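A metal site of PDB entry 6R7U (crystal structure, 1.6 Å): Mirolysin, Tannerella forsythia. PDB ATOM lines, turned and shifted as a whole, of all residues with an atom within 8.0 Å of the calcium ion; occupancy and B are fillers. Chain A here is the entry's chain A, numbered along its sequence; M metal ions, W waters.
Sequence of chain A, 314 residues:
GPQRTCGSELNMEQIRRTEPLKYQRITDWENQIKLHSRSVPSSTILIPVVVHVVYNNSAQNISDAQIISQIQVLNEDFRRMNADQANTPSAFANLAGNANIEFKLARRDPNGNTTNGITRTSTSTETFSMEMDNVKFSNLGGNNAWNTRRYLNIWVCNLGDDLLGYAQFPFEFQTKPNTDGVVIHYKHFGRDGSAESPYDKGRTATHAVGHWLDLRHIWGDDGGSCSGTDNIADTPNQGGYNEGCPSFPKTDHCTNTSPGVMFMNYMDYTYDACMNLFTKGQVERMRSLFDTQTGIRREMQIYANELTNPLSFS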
ATOM      1  N   HIS A 217     -12.903 -27.398  -6.088  1.00  0.00           N
ATOM      2  CA  HIS A 217     -12.329 -28.033  -7.269  1.00  0.00           C
ATOM      3  C   HIS A 217     -10.850 -27.797  -7.251  1.00  0.00           C
ATOM      4  O   HIS A 217     -10.409 -26.666  -7.037  1.00  0.00           O
ATOM      5  CB  HIS A 217     -12.936 -27.384  -8.494  1.00  0.00           C
ATOM      6  CG  HIS A 217     -14.339 -27.868  -8.644  1.00  0.00           C
ATOM      7  ND1 HIS A 217     -15.298 -27.094  -9.270  1.00  0.00           N
ATOM      8  CD2 HIS A 217     -14.911 -29.013  -8.204  1.00  0.00           C
ATOM      9  CE1 HIS A 217     -16.417 -27.833  -9.232  1.00  0.00           C
ATOM     10  NE2 HIS A 217     -16.220 -29.000  -8.613  1.00  0.00           N
ATOM     11  N   ILE A 218     -10.088 -28.825  -7.552  1.00  0.00           N
ATOM     12  CA  ILE A 218      -8.620 -28.759  -7.465  1.00  0.00           C
ATOM     13  C   ILE A 218      -7.995 -27.683  -8.387  1.00  0.00           C
ATOM     14  O   ILE A 218      -6.922 -27.111  -8.036  1.00  0.00           O
ATOM     15  CB  ILE A 218      -8.029 -30.165  -7.722  1.00  0.00           C
ATOM     16  CG1 ILE A 218      -6.561 -30.200  -7.493  1.00  0.00           C
ATOM     17  CG2 ILE A 218      -8.346 -30.640  -9.139  1.00  0.00           C
ATOM     18  CD1 ILE A 218      -5.999 -31.669  -7.355  1.00  0.00           C
ATOM     19  N   TRP A 219      -8.672 -27.370  -9.506  1.00  0.00           N
ATOM     20  CA  TRP A 219      -8.058 -26.387 -10.424  1.00  0.00           C
ATOM     21  C   TRP A 219      -8.381 -24.918 -10.062  1.00  0.00           C
ATOM     22  O   TRP A 219      -7.952 -23.991 -10.762  1.00  0.00           O
ATOM     23  CB  TRP A 219      -8.482 -26.653 -11.836  1.00  0.00           C
ATOM     24  CG  TRP A 219      -9.930 -26.386 -12.039  1.00  0.00           C
ATOM     25  CD1 TRP A 219     -10.493 -25.298 -12.648  1.00  0.00           C
ATOM     26  CD2 TRP A 219     -10.968 -27.332 -11.852  1.00  0.00           C
ATOM     27  NE1 TRP A 219     -11.859 -25.470 -12.731  1.00  0.00           N
ATOM     28  CE2 TRP A 219     -12.184 -26.708 -12.234  1.00  0.00           C
ATOM     29  CE3 TRP A 219     -10.992 -28.678 -11.455  1.00  0.00           C
ATOM     30  CZ2 TRP A 219     -13.409 -27.387 -12.205  1.00  0.00           C
ATOM     31  CZ3 TRP A 219     -12.223 -29.324 -11.359  1.00  0.00           C
ATOM     32  CH2 TRP A 219     -13.403 -28.702 -11.748  1.00  0.00           C
ATOM     33  N   GLY A 220      -9.202 -24.714  -9.031  1.00  0.00           N
ATOM     34  CA  GLY A 220      -9.434 -23.365  -8.560  1.00  0.00           C
ATOM     35  C   GLY A 220     -10.590 -22.594  -9.177  1.00  0.00           C
ATOM     36  O   GLY A 220     -10.777 -21.420  -8.858  1.00  0.00           O
ATOM     37  N   ASP A 221     -11.426 -23.258 -10.059  1.00  0.00           N
ATOM     38  CA  ASP A 221     -12.619 -22.629 -10.676  1.00  0.00           C
ATOM     39  C   ASP A 221     -12.296 -21.261 -11.313  1.00  0.00           C
ATOM     40  O   ASP A 221     -12.990 -20.251 -11.130  1.00  0.00           O
ATOM     41  CB  ASP A 221     -13.690 -22.516  -9.604  1.00  0.00           C
ATOM     42  CG  ASP A 221     -14.249 -23.858  -9.202  1.00  0.00           C
ATOM     43  OD1 ASP A 221     -14.596 -24.640 -10.089  1.00  0.00           O
ATOM     44  OD2 ASP A 221     -14.332 -24.115  -7.989  1.00  0.00           O
ATOM     45  N   ASP A 222     -11.202 -21.260 -12.058  1.00  0.00           N
ATOM     46  CA  ASP A 222     -10.725 -19.997 -12.593  1.00  0.00           C
ATOM     47  C   ASP A 222     -10.631 -20.022 -14.114  1.00  0.00           C
ATOM     48  O   ASP A 222      -9.828 -19.310 -14.699  1.00  0.00           O
ATOM     49  CB  ASP A 222      -9.357 -19.707 -11.969  1.00  0.00           C
ATOM     50  CG  ASP A 222      -8.340 -20.851 -12.076  1.00  0.00           C
ATOM     51  OD1 ASP A 222      -8.585 -21.816 -12.893  1.00  0.00           O
ATOM     52  OD2 ASP A 222      -7.330 -20.812 -11.362  1.00  0.00           O
ATOM     53  N   GLY A 223     -11.424 -20.894 -14.738  1.00  0.00           N
ATOM     54  CA  GLY A 223     -11.466 -20.977 -16.198  1.00  0.00           C
ATOM     55  C   GLY A 223     -10.198 -21.448 -16.886  1.00  0.00           C
ATOM     56  O   GLY A 223     -10.094 -21.394 -18.114  1.00  0.00           O
ATOM     57  N   GLY A 224      -9.240 -21.962 -16.140  1.00  0.00           N
ATOM     58  CA  GLY A 224      -8.036 -22.480 -16.766  1.00  0.00           C
ATOM     59  C   GLY A 224      -6.771 -21.749 -16.404  1.00  0.00           C
ATOM     60  O   GLY A 224      -5.670 -22.204 -16.741  1.00  0.00           O
ATOM     61  N   SER A 225      -6.902 -20.631 -15.695  1.00  0.00           N
ATOM     62  CA  SER A 225      -5.736 -19.846 -15.320  1.00  0.00           C
ATOM     63  C   SER A 225      -4.951 -20.504 -14.188  1.00  0.00           C
ATOM     64  O   SER A 225      -5.387 -21.520 -13.643  1.00  0.00           O
ATOM     65  CB  SER A 225      -6.185 -18.468 -14.891  1.00  0.00           C
ATOM     66  OG  SER A 225      -6.601 -18.486 -13.550  1.00  0.00           O
ATOM     67  N   CYS A 226      -3.842 -19.882 -13.790  1.00  0.00           N
ATOM     68  CA  CYS A 226      -3.042 -20.363 -12.661  1.00  0.00           C
ATOM     69  C   CYS A 226      -3.335 -19.516 -11.423  1.00  0.00           C
ATOM     70  O   CYS A 226      -2.697 -19.752 -10.391  1.00  0.00           O
ATOM     71  CB  CYS A 226      -1.564 -20.322 -13.031  1.00  0.00           C
ATOM     72  SG  CYS A 226      -1.161 -21.388 -14.448  1.00  0.00           S
ATOM     73  N   SER A 227      -4.320 -18.583 -11.503  1.00  0.00           N
ATOM     74  CA  SER A 227      -4.584 -17.625 -10.415  1.00  0.00           C
ATOM     75  C   SER A 227      -5.534 -18.093  -9.308  1.00  0.00           C
ATOM     76  O   SER A 227      -5.408 -17.604  -8.206  1.00  0.00           O
ATOM     77  CB  SER A 227      -5.121 -16.325 -10.992  1.00  0.00           C
ATOM     78  OG  SER A 227      -4.033 -15.653 -11.615  1.00  0.00           O
ATOM     79  N   GLY A 228      -6.521 -18.935  -9.623  1.00  0.00           N
ATOM     80  CA  GLY A 228      -7.437 -19.456  -8.622  1.00  0.00           C
ATOM     81  C   GLY A 228      -6.751 -20.513  -7.760  1.00  0.00           C
ATOM     82  O   GLY A 228      -5.657 -20.986  -8.085  1.00  0.00           O
ATOM     83  N   THR A 229      -7.374 -20.893  -6.649  1.00  0.00           N
ATOM     84  CA  THR A 229      -6.747 -21.844  -5.738  1.00  0.00           C
ATOM     85  C   THR A 229      -7.829 -22.725  -5.104  1.00  0.00           C
ATOM     86  O   THR A 229      -8.998 -22.312  -4.967  1.00  0.00           O
ATOM     87  CB  THR A 229      -5.987 -21.061  -4.628  1.00  0.00           C
ATOM     88  OG1 THR A 229      -5.316 -22.011  -3.766  1.00  0.00           O
ATOM     89  CG2 THR A 229      -6.935 -20.178  -3.792  1.00  0.00           C
ATOM     90  N   ASP A 230      -7.420 -23.895  -4.637  1.00  0.00           N
ATOM     91  CA  ASP A 230      -8.328 -24.731  -3.889  1.00  0.00           C
ATOM     92  C   ASP A 230      -7.936 -24.614  -2.397  1.00  0.00           C
ATOM     93  O   ASP A 230      -8.489 -25.317  -1.556  1.00  0.00           O
ATOM     94  CB  ASP A 230      -8.336 -26.188  -4.428  1.00  0.00           C
ATOM     95  CG  ASP A 230      -7.056 -26.990  -4.143  1.00  0.00           C
ATOM     96  OD1 ASP A 230      -5.990 -26.366  -3.884  1.00  0.00           O
ATOM     97  OD2 ASP A 230      -7.122 -28.237  -4.166  1.00  0.00           O
ATOM     98  N   PRO A 236      -1.282 -29.971  -6.358  1.00  0.00           N
ATOM     99  CA  PRO A 236      -0.551 -29.076  -7.267  1.00  0.00           C
ATOM    100  C   PRO A 236      -1.432 -28.026  -7.902  1.00  0.00           C
ATOM    101  O   PRO A 236      -2.574 -28.373  -8.339  1.00  0.00           O
ATOM    102  CB  PRO A 236      -0.031 -30.024  -8.351  1.00  0.00           C
ATOM    103  CG  PRO A 236       0.076 -31.390  -7.653  1.00  0.00           C
ATOM    104  CD  PRO A 236      -1.126 -31.395  -6.721  1.00  0.00           C
ATOM    105  N   ASN A 237      -0.857 -26.832  -8.112  1.00  0.00           N
ATOM    106  CA  ASN A 237      -1.570 -25.757  -8.847  1.00  0.00           C
ATOM    107  C   ASN A 237      -1.914 -26.311 -10.212  1.00  0.00           C
ATOM    108  O   ASN A 237      -1.119 -27.059 -10.792  1.00  0.00           O
ATOM    109  CB  ASN A 237      -0.757 -24.510  -8.944  1.00  0.00           C
ATOM    110  CG  ASN A 237      -1.543 -23.339  -9.475  1.00  0.00           C
ATOM    111  OD1 ASN A 237      -2.761 -23.396  -9.618  1.00  0.00           O
ATOM    112  ND2 ASN A 237      -0.860 -22.225  -9.743  1.00  0.00           N
ATOM    113  N   GLN A 238      -3.145 -26.104 -10.644  1.00  0.00           N
ATOM    114  CA  GLN A 238      -3.631 -26.689 -11.874  1.00  0.00           C
ATOM    115  C   GLN A 238      -4.378 -25.655 -12.679  1.00  0.00           C
ATOM    116  O   GLN A 238      -5.092 -24.841 -12.083  1.00  0.00           O
ATOM    117  CB  GLN A 238      -4.551 -27.837 -11.522  1.00  0.00           C
ATOM    118  CG  GLN A 238      -5.134 -28.668 -12.665  1.00  0.00           C
ATOM    119  CD  GLN A 238      -5.915 -29.845 -12.126  1.00  0.00           C
ATOM    120  OE1 GLN A 238      -5.427 -30.537 -11.242  1.00  0.00           O
ATOM    121  NE2 GLN A 238      -7.109 -30.134 -12.656  1.00  0.00           N
ATOM    122  N   GLY A 239      -4.243 -25.715 -14.006  1.00  0.00           N
ATOM    123  CA  GLY A 239      -4.920 -24.768 -14.884  1.00  0.00           C
ATOM    124  C   GLY A 239      -6.430 -24.896 -14.840  1.00  0.00           C
ATOM    125  O   GLY A 239      -7.127 -24.207 -14.086  1.00  0.00           O
ATOM    126  N   GLY A 240      -6.937 -25.751 -15.723  1.00  0.00           N
ATOM    127  CA  GLY A 240      -8.372 -26.008 -15.756  1.00  0.00           C
ATOM    128  C   GLY A 240      -8.661 -27.414 -15.253  1.00  0.00           C
ATOM    129  O   GLY A 240      -7.760 -28.108 -14.768  1.00  0.00           O
ATOM    130  N   TYR A 241      -9.910 -27.873 -15.397  1.00  0.00           N
ATOM    131  CA  TYR A 241     -10.219 -29.254 -14.983  1.00  0.00           C
ATOM    132  C   TYR A 241      -9.608 -30.255 -15.959  1.00  0.00           C
ATOM    133  O   TYR A 241      -9.284 -29.906 -17.091  1.00  0.00           O
ATOM    134  CB  TYR A 241     -11.741 -29.462 -14.906  1.00  0.00           C
ATOM    135  CG  TYR A 241     -12.505 -29.244 -16.204  1.00  0.00           C
ATOM    136  CD1 TYR A 241     -13.214 -28.073 -16.422  1.00  0.00           C
ATOM    137  CD2 TYR A 241     -12.551 -30.240 -17.172  1.00  0.00           C
ATOM    138  CE1 TYR A 241     -13.907 -27.877 -17.622  1.00  0.00           C
ATOM    139  CE2 TYR A 241     -13.274 -30.061 -18.357  1.00  0.00           C
ATOM    140  CZ  TYR A 241     -13.943 -28.876 -18.580  1.00  0.00           C
ATOM    141  OH  TYR A 241     -14.620 -28.704 -19.763  1.00  0.00           O
ATOM    142  N   ASP A 252       0.965 -29.245 -16.941  1.00  0.00           N
ATOM    143  CA  ASP A 252       0.229 -28.158 -17.601  1.00  0.00           C
ATOM    144  C   ASP A 252       0.982 -26.881 -17.316  1.00  0.00           C
ATOM    145  O   ASP A 252       2.052 -26.931 -16.677  1.00  0.00           O
ATOM    146  CB  ASP A 252      -1.264 -28.123 -17.190  1.00  0.00           C
ATOM    147  CG  ASP A 252      -1.618 -27.609 -15.800  1.00  0.00           C
ATOM    148  OD1 ASP A 252      -0.726 -27.093 -15.116  1.00  0.00           O
ATOM    149  OD2 ASP A 252      -2.824 -27.688 -15.420  1.00  0.00           O
ATOM    150  N   HIS A 253       0.440 -25.743 -17.770  1.00  0.00           N
ATOM    151  CA  HIS A 253       1.134 -24.452 -17.670  1.00  0.00           C
ATOM    152  C   HIS A 253       1.306 -24.015 -16.229  1.00  0.00           C
ATOM    153  O   HIS A 253       2.201 -23.211 -15.974  1.00  0.00           O
ATOM    154  CB  HIS A 253       0.440 -23.354 -18.516  1.00  0.00           C
ATOM    155  CG  HIS A 253      -1.000 -23.126 -18.156  1.00  0.00           C
ATOM    156  ND1 HIS A 253      -1.408 -21.963 -17.535  1.00  0.00           N
ATOM    157  CD2 HIS A 253      -2.079 -23.929 -18.326  1.00  0.00           C
ATOM    158  CE1 HIS A 253      -2.723 -22.084 -17.364  1.00  0.00           C
ATOM    159  NE2 HIS A 253      -3.166 -23.254 -17.828  1.00  0.00           N
ATOM    160  N   CYS A 254       0.512 -24.558 -15.300  1.00  0.00           N
ATOM    161  CA  CYS A 254       0.620 -24.203 -13.880  1.00  0.00           C
ATOM    162  C   CYS A 254       1.669 -25.081 -13.158  1.00  0.00           C
ATOM    163  O   CYS A 254       2.469 -24.555 -12.375  1.00  0.00           O
ATOM    164  CB  CYS A 254      -0.735 -24.258 -13.188  1.00  0.00           C
ATOM    165  SG  CYS A 254      -2.007 -23.196 -13.932  1.00  0.00           S
HETATM  166 CA    CA M   1      -6.546 -22.940 -12.220  1.00  0.00          CA
HETATM  167  O   HOH W   1      -5.093 -22.554 -10.423  1.00  0.00           O
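The side-chain hydroxyl (OG) of Ser 225 sits at hydrogen-bond distance from the backbone NH (N) of Ser 227 (3.1 Å).
The backbone NH (N) of Gly 239 sits at hydrogen-bond distance from the side-chain sulfur (SG) of Cys 254, 3.4 Å away.
N of Gly 239 is in hydrogen-bond range of OD2 of Asp 252 (2.8 Å).
The side-chain amide nitrogen (NE2) of Gln 238 lies within hydrogen-bond range of the backbone carbonyl oxygen (O) of Gly 240, 3.0 Å away.
N of Gly 224 sits close to OD1 of Asp 222, at 3.3 Å.
The side-chain carboxylate of Asp 222 lies close to the backbone NH of Gly 228 (2.7 Å).
SG of Cys 226 forms a disulfide with SG of Cys 254 (2.1 Å).
Within 4 Å of the calcium ion: Trp 219, Asp 222, Ser 225, Gln 238 and Gly 239.
Along chain A the residues within 4 Å of the calcium ion span positions 219 to 239.
The nearest printed residue that does not touch the calcium ion is Gly 224 (4.4 Å).
The calcium ion is bound by O of Trp 219 (2.3 Å), O of Ser 225 (2.3 Å), O of Gly 239 (2.3 Å), water W1 (2.3 Å), O of Gln 238 (2.4 Å), OD1 of Asp 222 (2.4 Å) and OD2 of Asp 222 (2.4 Å).
The calcium ion has seven donor atoms within binding distance.
Water W1 lies within hydrogen-bond range of OD1 of Asn 237 (2.6 Å) and O of Gly 228 (2.9 Å).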
